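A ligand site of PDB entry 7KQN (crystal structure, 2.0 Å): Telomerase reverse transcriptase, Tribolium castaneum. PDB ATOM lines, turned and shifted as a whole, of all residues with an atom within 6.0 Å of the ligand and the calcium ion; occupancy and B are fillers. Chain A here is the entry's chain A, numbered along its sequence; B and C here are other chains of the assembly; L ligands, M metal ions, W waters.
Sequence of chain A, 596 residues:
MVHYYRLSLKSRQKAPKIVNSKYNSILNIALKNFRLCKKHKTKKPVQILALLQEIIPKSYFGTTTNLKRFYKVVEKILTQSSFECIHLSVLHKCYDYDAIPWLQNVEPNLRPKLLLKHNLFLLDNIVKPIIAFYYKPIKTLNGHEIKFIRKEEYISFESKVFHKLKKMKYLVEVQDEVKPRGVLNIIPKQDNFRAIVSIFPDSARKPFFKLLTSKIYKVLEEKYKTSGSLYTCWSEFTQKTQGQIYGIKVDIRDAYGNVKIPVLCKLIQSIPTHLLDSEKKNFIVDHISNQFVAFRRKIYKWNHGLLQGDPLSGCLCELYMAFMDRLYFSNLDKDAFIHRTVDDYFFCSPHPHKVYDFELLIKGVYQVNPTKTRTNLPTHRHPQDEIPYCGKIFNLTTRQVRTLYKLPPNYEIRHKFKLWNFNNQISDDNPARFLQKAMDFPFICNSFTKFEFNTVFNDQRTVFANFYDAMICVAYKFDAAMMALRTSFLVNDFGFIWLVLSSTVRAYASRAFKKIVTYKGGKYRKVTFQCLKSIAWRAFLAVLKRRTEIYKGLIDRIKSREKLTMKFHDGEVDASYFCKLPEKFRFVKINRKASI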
ATOM      1  N   LEU A 141      -4.715   8.260  -5.384  1.00  0.00           N
ATOM      2  CA  LEU A 141      -6.005   8.019  -6.027  1.00  0.00           C
ATOM      3  C   LEU A 141      -7.142   8.263  -5.031  1.00  0.00           C
ATOM      4  O   LEU A 141      -8.312   7.949  -5.338  1.00  0.00           O
ATOM      5  CB  LEU A 141      -6.122   6.603  -6.604  1.00  0.00           C
ATOM      6  CG  LEU A 141      -5.409   6.316  -7.931  1.00  0.00           C
ATOM      7  CD1 LEU A 141      -5.872   7.180  -9.096  1.00  0.00           C
ATOM      8  CD2 LEU A 141      -3.897   6.364  -7.789  1.00  0.00           C
ATOM      9  N   LYS A 189      -2.135   0.231  -4.069  1.00  0.00           N
ATOM     10  CA  LYS A 189      -3.603   0.292  -3.806  1.00  0.00           C
ATOM     11  C   LYS A 189      -3.939  -0.294  -2.434  1.00  0.00           C
ATOM     12  O   LYS A 189      -4.375  -1.464  -2.405  1.00  0.00           O
ATOM     13  CB  LYS A 189      -4.369  -0.453  -4.901  1.00  0.00           C
ATOM     14  CG  LYS A 189      -5.419   0.354  -5.640  1.00  0.00           C
ATOM     15  CD  LYS A 189      -6.827  -0.114  -5.370  1.00  0.00           C
ATOM     16  CE  LYS A 189      -6.894  -1.548  -4.903  1.00  0.00           C
ATOM     17  NZ  LYS A 189      -7.820  -2.350  -5.748  1.00  0.00           N
ATOM     18  N   ASN A 192      -2.329  -3.368  -1.696  1.00  0.00           N
ATOM     19  CA  ASN A 192      -2.395  -4.177  -2.937  1.00  0.00           C
ATOM     20  C   ASN A 192      -1.859  -3.281  -4.058  1.00  0.00           C
ATOM     21  O   ASN A 192      -1.193  -2.280  -3.742  1.00  0.00           O
ATOM     22  CB  ASN A 192      -3.809  -4.679  -3.225  1.00  0.00           C
ATOM     23  CG  ASN A 192      -4.600  -5.004  -1.970  1.00  0.00           C
ATOM     24  OD1 ASN A 192      -5.492  -4.254  -1.585  1.00  0.00           O
ATOM     25  ND2 ASN A 192      -4.268  -6.109  -1.333  1.00  0.00           N
ATOM     26  N   ARG A 194      -2.476  -1.803  -8.441  1.00  0.00           N
ATOM     27  CA  ARG A 194      -3.341  -1.743  -9.640  1.00  0.00           C
ATOM     28  C   ARG A 194      -2.417  -1.665 -10.860  1.00  0.00           C
ATOM     29  O   ARG A 194      -1.777  -0.611 -11.034  1.00  0.00           O
ATOM     30  CB  ARG A 194      -4.325  -0.574  -9.618  1.00  0.00           C
ATOM     31  CG  ARG A 194      -5.315  -0.600 -10.768  1.00  0.00           C
ATOM     32  CD  ARG A 194      -6.321   0.528 -10.763  1.00  0.00           C
ATOM     33  NE  ARG A 194      -7.173   0.526  -9.595  1.00  0.00           N
ATOM     34  CZ  ARG A 194      -8.243  -0.240  -9.447  1.00  0.00           C
ATOM     35  NH1 ARG A 194      -8.614  -1.084 -10.398  1.00  0.00           N
ATOM     36  NH2 ARG A 194      -8.957  -0.162  -8.330  1.00  0.00           N
ATOM     37  N   ILE A 196      -1.865  -1.013 -14.494  1.00  0.00           N
ATOM     38  CA  ILE A 196      -2.558  -0.324 -15.572  1.00  0.00           C
ATOM     39  C   ILE A 196      -1.589  -0.156 -16.723  1.00  0.00           C
ATOM     40  O   ILE A 196      -0.366  -0.200 -16.541  1.00  0.00           O
ATOM     41  CB  ILE A 196      -3.091   1.068 -15.149  1.00  0.00           C
ATOM     42  CG1 ILE A 196      -1.918   2.029 -14.893  1.00  0.00           C
ATOM     43  CG2 ILE A 196      -3.995   0.982 -13.925  1.00  0.00           C
ATOM     44  CD1 ILE A 196      -2.299   3.440 -14.984  1.00  0.00           C
ATOM     45  N   ASP A 251     -18.291  -7.757  -4.542  1.00  0.00           N
ATOM     46  CA  ASP A 251     -17.360  -7.184  -5.506  1.00  0.00           C
ATOM     47  C   ASP A 251     -16.543  -8.301  -6.135  1.00  0.00           C
ATOM     48  O   ASP A 251     -16.068  -9.186  -5.416  1.00  0.00           O
ATOM     49  CB  ASP A 251     -16.401  -6.185  -4.838  1.00  0.00           C
ATOM     50  CG  ASP A 251     -15.361  -5.659  -5.823  1.00  0.00           C
ATOM     51  OD1 ASP A 251     -14.242  -6.243  -5.854  1.00  0.00           O
ATOM     52  OD2 ASP A 251     -15.593  -4.625  -6.459  1.00  0.00           O
ATOM     53  N   ILE A 252     -16.359  -8.280  -7.456  1.00  0.00           N
ATOM     54  CA  ILE A 252     -15.527  -9.297  -8.108  1.00  0.00           C
ATOM     55  C   ILE A 252     -14.062  -8.964  -7.886  1.00  0.00           C
ATOM     56  O   ILE A 252     -13.643  -7.814  -8.048  1.00  0.00           O
ATOM     57  CB  ILE A 252     -15.853  -9.415  -9.597  1.00  0.00           C
ATOM     58  CG1 ILE A 252     -17.303  -9.856  -9.771  1.00  0.00           C
ATOM     59  CG2 ILE A 252     -14.901 -10.436 -10.303  1.00  0.00           C
ATOM     60  CD1 ILE A 252     -17.781  -9.764 -11.219  1.00  0.00           C
ATOM     61  N   ARG A 253     -13.271  -9.967  -7.533  1.00  0.00           N
ATOM     62  CA  ARG A 253     -11.844  -9.749  -7.414  1.00  0.00           C
ATOM     63  C   ARG A 253     -11.198  -9.555  -8.805  1.00  0.00           C
ATOM     64  O   ARG A 253     -11.462 -10.337  -9.724  1.00  0.00           O
ATOM     65  CB  ARG A 253     -11.210 -10.923  -6.687  1.00  0.00           C
ATOM     66  CG  ARG A 253      -9.713 -10.935  -6.693  1.00  0.00           C
ATOM     67  CD  ARG A 253      -9.195 -12.087  -5.880  1.00  0.00           C
ATOM     68  NE  ARG A 253      -9.142 -11.704  -4.473  1.00  0.00           N
ATOM     69  CZ  ARG A 253      -9.260 -12.553  -3.454  1.00  0.00           C
ATOM     70  NH1 ARG A 253      -9.417 -13.854  -3.700  1.00  0.00           N
ATOM     71  NH2 ARG A 253      -9.211 -12.111  -2.205  1.00  0.00           N
ATOM     72  N   ASP A 254     -10.366  -8.518  -8.963  1.00  0.00           N
ATOM     73  CA  ASP A 254      -9.554  -8.364 -10.182  1.00  0.00           C
ATOM     74  C   ASP A 254     -10.427  -8.484 -11.426  1.00  0.00           C
ATOM     75  O   ASP A 254     -10.216  -9.347 -12.281  1.00  0.00           O
ATOM     76  CB  ASP A 254      -8.453  -9.441 -10.209  1.00  0.00           C
ATOM     77  CG  ASP A 254      -7.326  -9.161 -11.231  1.00  0.00           C
ATOM     78  OD1 ASP A 254      -7.386  -8.166 -11.998  1.00  0.00           O
ATOM     79  OD2 ASP A 254      -6.350  -9.959 -11.212  1.00  0.00           O
ATOM     80  N   ALA A 255     -11.441  -7.624 -11.493  1.00  0.00           N
ATOM     81  CA  ALA A 255     -12.530  -7.857 -12.450  1.00  0.00           C
ATOM     82  C   ALA A 255     -12.024  -7.944 -13.897  1.00  0.00           C
ATOM     83  O   ALA A 255     -12.309  -8.926 -14.590  1.00  0.00           O
ATOM     84  CB  ALA A 255     -13.571  -6.758 -12.329  1.00  0.00           C
ATOM     85  N   TYR A 256     -11.282  -6.936 -14.377  1.00  0.00           N
ATOM     86  CA  TYR A 256     -10.819  -6.977 -15.773  1.00  0.00           C
ATOM     87  C   TYR A 256      -9.894  -8.155 -16.001  1.00  0.00           C
ATOM     88  O   TYR A 256      -9.926  -8.773 -17.080  1.00  0.00           O
ATOM     89  CB  TYR A 256     -10.071  -5.693 -16.160  1.00  0.00           C
ATOM     90  CG  TYR A 256     -10.910  -4.486 -16.520  1.00  0.00           C
ATOM     91  CD1 TYR A 256     -12.234  -4.369 -16.064  1.00  0.00           C
ATOM     92  CD2 TYR A 256     -10.367  -3.437 -17.261  1.00  0.00           C
ATOM     93  CE1 TYR A 256     -12.994  -3.240 -16.367  1.00  0.00           C
ATOM     94  CE2 TYR A 256     -11.110  -2.332 -17.578  1.00  0.00           C
ATOM     95  CZ  TYR A 256     -12.420  -2.222 -17.123  1.00  0.00           C
ATOM     96  OH  TYR A 256     -13.138  -1.097 -17.448  1.00  0.00           O
ATOM     97  N   GLY A 257      -9.041  -8.457 -15.024  1.00  0.00           N
ATOM     98  CA  GLY A 257      -8.090  -9.527 -15.154  1.00  0.00           C
ATOM     99  C   GLY A 257      -8.733 -10.884 -15.281  1.00  0.00           C
ATOM    100  O   GLY A 257      -8.127 -11.796 -15.862  1.00  0.00           O
ATOM    101  N   GLN A 308      -6.248  -3.019 -17.979  1.00  0.00           N
ATOM    102  CA  GLN A 308      -6.855  -1.826 -17.378  1.00  0.00           C
ATOM    103  C   GLN A 308      -6.107  -0.575 -17.840  1.00  0.00           C
ATOM    104  O   GLN A 308      -4.908  -0.451 -17.626  1.00  0.00           O
ATOM    105  CB  GLN A 308      -6.806  -1.887 -15.855  1.00  0.00           C
ATOM    106  CG  GLN A 308      -7.528  -3.072 -15.243  1.00  0.00           C
ATOM    107  CD  GLN A 308      -7.238  -3.153 -13.751  1.00  0.00           C
ATOM    108  OE1 GLN A 308      -7.527  -2.211 -13.021  1.00  0.00           O
ATOM    109  NE2 GLN A 308      -6.626  -4.242 -13.315  1.00  0.00           N
ATOM    110  N   GLY A 309      -6.851   0.363 -18.418  1.00  0.00           N
ATOM    111  CA  GLY A 309      -6.276   1.568 -19.004  1.00  0.00           C
ATOM    112  C   GLY A 309      -6.325   1.577 -20.509  1.00  0.00           C
ATOM    113  O   GLY A 309      -5.940   2.581 -21.113  1.00  0.00           O
ATOM    114  N   ASP A 310      -6.724   0.477 -21.126  1.00  0.00           N
ATOM    115  CA  ASP A 310      -6.959   0.513 -22.569  1.00  0.00           C
ATOM    116  C   ASP A 310      -8.372   1.030 -22.810  1.00  0.00           C
ATOM    117  O   ASP A 310      -9.305   0.593 -22.129  1.00  0.00           O
ATOM    118  CB  ASP A 310      -6.805  -0.875 -23.200  1.00  0.00           C
ATOM    119  CG  ASP A 310      -7.105  -0.880 -24.688  1.00  0.00           C
ATOM    120  OD1 ASP A 310      -6.194  -0.529 -25.465  1.00  0.00           O
ATOM    121  OD2 ASP A 310      -8.268  -1.144 -25.087  1.00  0.00           O
ATOM    122  N   VAL A 342     -20.575  -2.215 -13.000  1.00  0.00           N
ATOM    123  CA  VAL A 342     -19.304  -2.870 -13.423  1.00  0.00           C
ATOM    124  C   VAL A 342     -19.230  -4.256 -12.760  1.00  0.00           C
ATOM    125  O   VAL A 342     -19.983  -5.135 -13.192  1.00  0.00           O
ATOM    126  CB  VAL A 342     -18.055  -1.996 -13.225  1.00  0.00           C
ATOM    127  CG1 VAL A 342     -16.822  -2.597 -13.878  1.00  0.00           C
ATOM    128  CG2 VAL A 342     -18.282  -0.585 -13.737  1.00  0.00           C
ATOM    129  N   ASP A 343     -18.342  -4.440 -11.791  1.00  0.00           N
ATOM    130  CA  ASP A 343     -18.147  -5.758 -11.129  1.00  0.00           C
ATOM    131  C   ASP A 343     -18.816  -5.807  -9.747  1.00  0.00           C
ATOM    132  O   ASP A 343     -18.534  -6.752  -8.999  1.00  0.00           O
ATOM    133  CB  ASP A 343     -16.661  -6.062 -10.981  1.00  0.00           C
ATOM    134  CG  ASP A 343     -15.906  -5.045 -10.149  1.00  0.00           C
ATOM    135  OD1 ASP A 343     -16.177  -3.844 -10.310  1.00  0.00           O
ATOM    136  OD2 ASP A 343     -15.042  -5.462  -9.351  1.00  0.00           O
ATOM    137  N   ASP A 344     -19.640  -4.803  -9.403  1.00  0.00           N
ATOM    138  CA  ASP A 344     -20.244  -4.764  -8.044  1.00  0.00           C
ATOM    139  C   ASP A 344     -21.732  -5.083  -8.101  1.00  0.00           C
ATOM    140  O   ASP A 344     -22.434  -4.443  -8.888  1.00  0.00           O
ATOM    141  CB  ASP A 344     -19.993  -3.422  -7.348  1.00  0.00           C
ATOM    142  CG  ASP A 344     -18.546  -3.263  -6.928  1.00  0.00           C
ATOM    143  OD1 ASP A 344     -17.838  -4.273  -6.931  1.00  0.00           O
ATOM    144  OD2 ASP A 344     -18.154  -2.131  -6.602  1.00  0.00           O
ATOM    145  N   ASN A 369     -14.195 -10.743  -4.107  1.00  0.00           N
ATOM    146  CA  ASN A 369     -13.298 -10.063  -3.181  1.00  0.00           C
ATOM    147  C   ASN A 369     -13.979 -10.054  -1.815  1.00  0.00           C
ATOM    148  O   ASN A 369     -14.864  -9.224  -1.579  1.00  0.00           O
ATOM    149  CB  ASN A 369     -13.003  -8.649  -3.661  1.00  0.00           C
ATOM    150  CG  ASN A 369     -11.998  -7.928  -2.810  1.00  0.00           C
ATOM    151  OD1 ASN A 369     -11.542  -8.430  -1.787  1.00  0.00           O
ATOM    152  ND2 ASN A 369     -11.630  -6.728  -3.235  1.00  0.00           N
ATOM    153  N   LYS A 372     -14.556  -6.804   0.484  1.00  0.00           N
ATOM    154  CA  LYS A 372     -15.528  -5.793   0.101  1.00  0.00           C
ATOM    155  C   LYS A 372     -16.972  -6.217   0.348  1.00  0.00           C
ATOM    156  O   LYS A 372     -17.888  -5.414   0.126  1.00  0.00           O
ATOM    157  CB  LYS A 372     -15.345  -5.440  -1.379  1.00  0.00           C
ATOM    158  CG  LYS A 372     -14.016  -4.722  -1.704  1.00  0.00           C
ATOM    159  CD  LYS A 372     -14.064  -4.074  -3.097  1.00  0.00           C
ATOM    160  CE  LYS A 372     -12.665  -3.826  -3.669  1.00  0.00           C
ATOM    161  NZ  LYS A 372     -12.698  -3.140  -5.022  1.00  0.00           N
ATOM    162  P     C B  10      -2.862   9.908 -16.188  1.00  0.00           P
ATOM    163  OP1   C B  10      -1.913  10.885 -16.675  1.00  0.00           O
ATOM    164  OP2   C B  10      -3.998  10.359 -15.342  1.00  0.00           O
ATOM    165  O5'   C B  10      -3.534   9.107 -17.401  1.00  0.00           O
ATOM    166  C5'   C B  10      -2.728   8.473 -18.393  1.00  0.00           C
ATOM    167  C4'   C B  10      -3.300   7.146 -18.813  1.00  0.00           C
ATOM    168  O4'   C B  10      -3.080   6.156 -17.771  1.00  0.00           O
ATOM    169  C3'   C B  10      -4.809   7.101 -19.022  1.00  0.00           C
ATOM    170  O3'   C B  10      -5.209   7.637 -20.269  1.00  0.00           O
ATOM    171  C2'   C B  10      -5.107   5.622 -18.851  1.00  0.00           C
ATOM    172  O2'   C B  10      -4.699   4.866 -20.002  1.00  0.00           O
ATOM    173  C1'   C B  10      -4.170   5.274 -17.699  1.00  0.00           C
ATOM    174  N1    C B  10      -4.810   5.455 -16.382  1.00  0.00           N
ATOM    175  C2    C B  10      -5.726   4.506 -15.944  1.00  0.00           C
ATOM    176  O2    C B  10      -5.982   3.524 -16.672  1.00  0.00           O
ATOM    177  N3    C B  10      -6.322   4.656 -14.740  1.00  0.00           N
ATOM    178  C4    C B  10      -6.016   5.714 -13.986  1.00  0.00           C
ATOM    179  N4    C B  10      -6.638   5.835 -12.808  1.00  0.00           N
ATOM    180  C5    C B  10      -5.077   6.710 -14.424  1.00  0.00           C
ATOM    181  C6    C B  10      -4.511   6.544 -15.611  1.00  0.00           C
ATOM    182  P     C B  11      -6.644   8.300 -20.439  1.00  0.00           P
ATOM    183  OP1   C B  11      -6.739   8.878 -21.794  1.00  0.00           O
ATOM    184  OP2   C B  11      -7.006   9.067 -19.211  1.00  0.00           O
ATOM    185  O5'   C B  11      -7.652   7.072 -20.361  1.00  0.00           O
ATOM    186  C5'   C B  11      -7.509   5.927 -21.199  1.00  0.00           C
ATOM    187  C4'   C B  11      -8.554   4.885 -20.856  1.00  0.00           C
ATOM    188  O4'   C B  11      -8.319   4.364 -19.511  1.00  0.00           O
ATOM    189  C3'   C B  11      -9.983   5.397 -20.784  1.00  0.00           C
ATOM    190  O3'   C B  11     -10.550   5.544 -22.069  1.00  0.00           O
ATOM    191  C2'   C B  11     -10.661   4.336 -19.911  1.00  0.00           C
ATOM    192  O2'   C B  11     -10.883   3.141 -20.649  1.00  0.00           O
ATOM    193  C1'   C B  11      -9.542   4.018 -18.912  1.00  0.00           C
ATOM    194  N1    C B  11      -9.685   4.696 -17.595  1.00  0.00           N
ATOM    195  C2    C B  11     -10.643   4.182 -16.711  1.00  0.00           C
ATOM    196  O2    C B  11     -11.340   3.221 -17.057  1.00  0.00           O
ATOM    197  N3    C B  11     -10.799   4.727 -15.483  1.00  0.00           N
ATOM    198  C4    C B  11     -10.049   5.752 -15.100  1.00  0.00           C
ATOM    199  N4    C B  11     -10.289   6.229 -13.886  1.00  0.00           N
ATOM    200  C5    C B  11      -9.056   6.320 -15.981  1.00  0.00           C
ATOM    201  C6    C B  11      -8.896   5.765 -17.200  1.00  0.00           C
ATOM    202  P    DG C   7     -17.915   2.201  -6.260  1.00  0.00           P
ATOM    203  OP1  DG C   7     -18.569   1.261  -5.363  1.00  0.00           O
ATOM    204  OP2  DG C   7     -16.783   3.045  -5.841  1.00  0.00           O
ATOM    205  O5'  DG C   7     -17.332   1.379  -7.551  1.00  0.00           O
ATOM    206  C5'  DG C   7     -18.089   0.315  -8.116  1.00  0.00           C
ATOM    207  C4'  DG C   7     -17.387  -0.184  -9.362  1.00  0.00           C
ATOM    208  O4'  DG C   7     -17.295   0.887 -10.330  1.00  0.00           O
ATOM    209  C3'  DG C   7     -15.963  -0.577  -9.147  1.00  0.00           C
ATOM    210  O3'  DG C   7     -15.906  -1.891  -8.538  1.00  0.00           O
ATOM    211  C2'  DG C   7     -15.441  -0.541 -10.577  1.00  0.00           C
ATOM    212  C1'  DG C   7     -16.137   0.704 -11.122  1.00  0.00           C
ATOM    213  N9   DG C   7     -15.260   1.910 -11.057  1.00  0.00           N
ATOM    214  C8   DG C   7     -15.071   2.766 -10.005  1.00  0.00           C
ATOM    215  N7   DG C   7     -14.178   3.696 -10.273  1.00  0.00           N
ATOM    216  C5   DG C   7     -13.751   3.436 -11.575  1.00  0.00           C
ATOM    217  C6   DG C   7     -12.778   4.110 -12.398  1.00  0.00           C
ATOM    218  O6   DG C   7     -12.094   5.109 -12.137  1.00  0.00           O
ATOM    219  N1   DG C   7     -12.661   3.522 -13.639  1.00  0.00           N
ATOM    220  C2   DG C   7     -13.340   2.408 -14.056  1.00  0.00           C
ATOM    221  N2   DG C   7     -13.082   1.972 -15.296  1.00  0.00           N
ATOM    222  N3   DG C   7     -14.243   1.762 -13.297  1.00  0.00           N
ATOM    223  C4   DG C   7     -14.407   2.354 -12.076  1.00  0.00           C
HETATM  224  P1  LIG L   1      -9.947  -5.876  -6.466  1.00  0.00           P
HETATM  225  O1  LIG L   1      -9.069  -4.939  -5.667  1.00  0.00           O
HETATM  226  O2  LIG L   1     -11.423  -5.518  -6.414  1.00  0.00           O
HETATM  227  O3  LIG L   1      -9.698  -7.339  -6.176  1.00  0.00           O
HETATM  228  O4  LIG L   1      -9.367  -5.530  -8.070  1.00  0.00           O
HETATM  229  P2  LIG L   1     -10.214  -4.963  -9.268  1.00  0.00           P
HETATM  230  O5  LIG L   1      -9.351  -4.879 -10.491  1.00  0.00           O
HETATM  231  O6  LIG L   1     -11.598  -5.487  -9.389  1.00  0.00           O
HETATM  232  O7  LIG L   1     -10.507  -3.243  -9.099  1.00  0.00           O
HETATM  233  P3  LIG L   1     -11.827  -2.502  -8.734  1.00  0.00           P
HETATM  234  O8  LIG L   1     -11.659  -1.070  -8.332  1.00  0.00           O
HETATM  235  O9  LIG L   1     -12.959  -3.268  -8.132  1.00  0.00           O
HETATM  236  O10 LIG L   1     -12.707  -2.173 -10.291  1.00  0.00           O
HETATM  237  C1  LIG L   1     -13.121  -3.178 -11.040  1.00  0.00           C
HETATM  238  C2  LIG L   1     -12.621  -2.958 -12.501  1.00  0.00           C
HETATM  239  O11 LIG L   1     -12.844  -1.586 -12.866  1.00  0.00           O
HETATM  240  C3  LIG L   1     -11.106  -3.130 -12.560  1.00  0.00           C
HETATM  241  O12 LIG L   1     -10.746  -4.450 -12.858  1.00  0.00           O
HETATM  242  C4  LIG L   1     -10.797  -2.250 -13.712  1.00  0.00           C
HETATM  243  C5  LIG L   1     -11.819  -1.091 -13.629  1.00  0.00           C
HETATM  244  N1  LIG L   1     -11.188   0.062 -12.960  1.00  0.00           N
HETATM  245  C6  LIG L   1     -11.432   0.459 -11.635  1.00  0.00           C
HETATM  246  N2  LIG L   1     -10.704   1.530 -11.293  1.00  0.00           N
HETATM  247  C7  LIG L   1      -9.928   1.843 -12.417  1.00  0.00           C
HETATM  248  C8  LIG L   1      -8.973   2.816 -12.751  1.00  0.00           C
HETATM  249  O13 LIG L   1      -8.610   3.747 -11.829  1.00  0.00           O
HETATM  250  N3  LIG L   1      -8.378   2.871 -13.957  1.00  0.00           N
HETATM  251  C9  LIG L   1      -8.756   1.911 -14.884  1.00  0.00           C
HETATM  252  N4  LIG L   1      -8.147   1.956 -16.143  1.00  0.00           N
HETATM  253  N5  LIG L   1      -9.667   0.917 -14.710  1.00  0.00           N
HETATM  254  C10 LIG L   1     -10.226   0.912 -13.470  1.00  0.00           C
HETATM  255 CA    CA M   1     -13.360  -5.578  -7.839  1.00  0.00          CA
HETATM  256  O   HOH W   1     -12.915   1.119  -8.230  1.00  0.00           O
HETATM  257  O   HOH W   2      -8.437  -8.877  -4.223  1.00  0.00           O
HETATM  258  O   HOH W   3     -14.672  -1.932  -6.081  1.00  0.00           O
HETATM  259  O   HOH W   4      -6.975  -7.596  -7.159  1.00  0.00           O
HETATM  260  O   HOH W   5     -10.633  -1.183  -5.634  1.00  0.00           O
HETATM  261  O   HOH W   6     -11.007   2.890  -8.914  1.00  0.00           O
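Water W2 bridges an oxygen (O3) of the ligand (2.8 Å) and the guanidinium group (NE) of Arg 253 (2.9 Å). Water W3 bridges the side-chain amino group (NZ) of Lys 372 (2.5 Å) and O3' of DG 7 of chain C (2.7 Å).
The side-chain carboxylate (OD2) of Asp 251 lies close to the side-chain amino group (NZ) of Lys 372, 3.6 Å away. The side-chain carboxylate (OD1) of Asp 254 lies within hydrogen-bond range of the backbone NH (N) of Gly 257, at 3.5 Å. NH1 of Arg 194 lies within hydrogen-bond range of OE1 of Gln 308, 3.1 Å away. N of Asn 369 is in hydrogen-bond range of O of Asp 251. The side-chain carboxylate (OD1) of Asp 343 sits close to O3' of DG 7 of chain C (2.7 Å). OD1 of Asn 192 sits close to O of Lys 189, at 3.1 Å.
An oxygen (O2) of the ligand sits close to the side-chain amide nitrogen (ND2) of Asn 369 (3.4 Å). The side-chain amino group (NZ) of Lys 372 lies close to an oxygen (O2) of the ligand (3.0 Å). The backbone NH of Asp 254 sits at hydrogen-bond distance from an oxygen (O3) of the ligand (3.1 Å). A nitrogen (N3) of the ligand sits at hydrogen-bond distance from N3 of C 11 of chain B, at 3.4 Å. The backbone NH of Ala 255 lies close to an oxygen (O6) of the ligand (3.0 Å). O2 of C 10 of chain B sits at hydrogen-bond distance from a nitrogen (N4) of the ligand, at 2.7 Å. The guanidinium group (NH2) of Arg 194 lies within salt-bridge range of an oxygen (O8) of the ligand, 2.9 Å away. An oxygen (O1) of the ligand lies within salt-bridge range of the side-chain amino group (NZ) of Lys 189, at 2.9 Å. An oxygen (O12) of the ligand sits at hydrogen-bond distance from the backbone NH (N) of Tyr 256 (3.0 Å).
N of Gly 309 sits close to N4 of the ligand (3.1 Å). O3' of DG 7 of chain C sits close to an oxygen (O9) of the ligand, 3.3 Å away. Residues that only touch the ligand: Arg 253 (3.5 Å) and Gln 308 (3.3 Å). Within 4 Å of the ligand: Lys 189, Arg 194, Asp 251, Ile 252, Arg 253, Asp 254, Ala 255, Tyr 256, Gln 308, Gly 309, Asp 343, Asn 369, Lys 372, C 10 of chain B, C 11 of chain B and DG 7 of chain C. The nearest printed residue that does not touch the ligand is Val 342 (4.2 Å).
Residues that only touch the calcium ion: Lys 372.
The calcium ion is bound by O of Ile 252 (2.3 Å), OD2 of Asp 343 (2.3 Å), OD1 of Asp 251 (2.3 Å), O6 of the ligand (2.3 Å), O9 of the ligand (2.4 Å), O2 of the ligand (2.4 Å) and OD2 of Asp 251 (2.8 Å). The calcium ion has seven donor atoms within binding distance.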
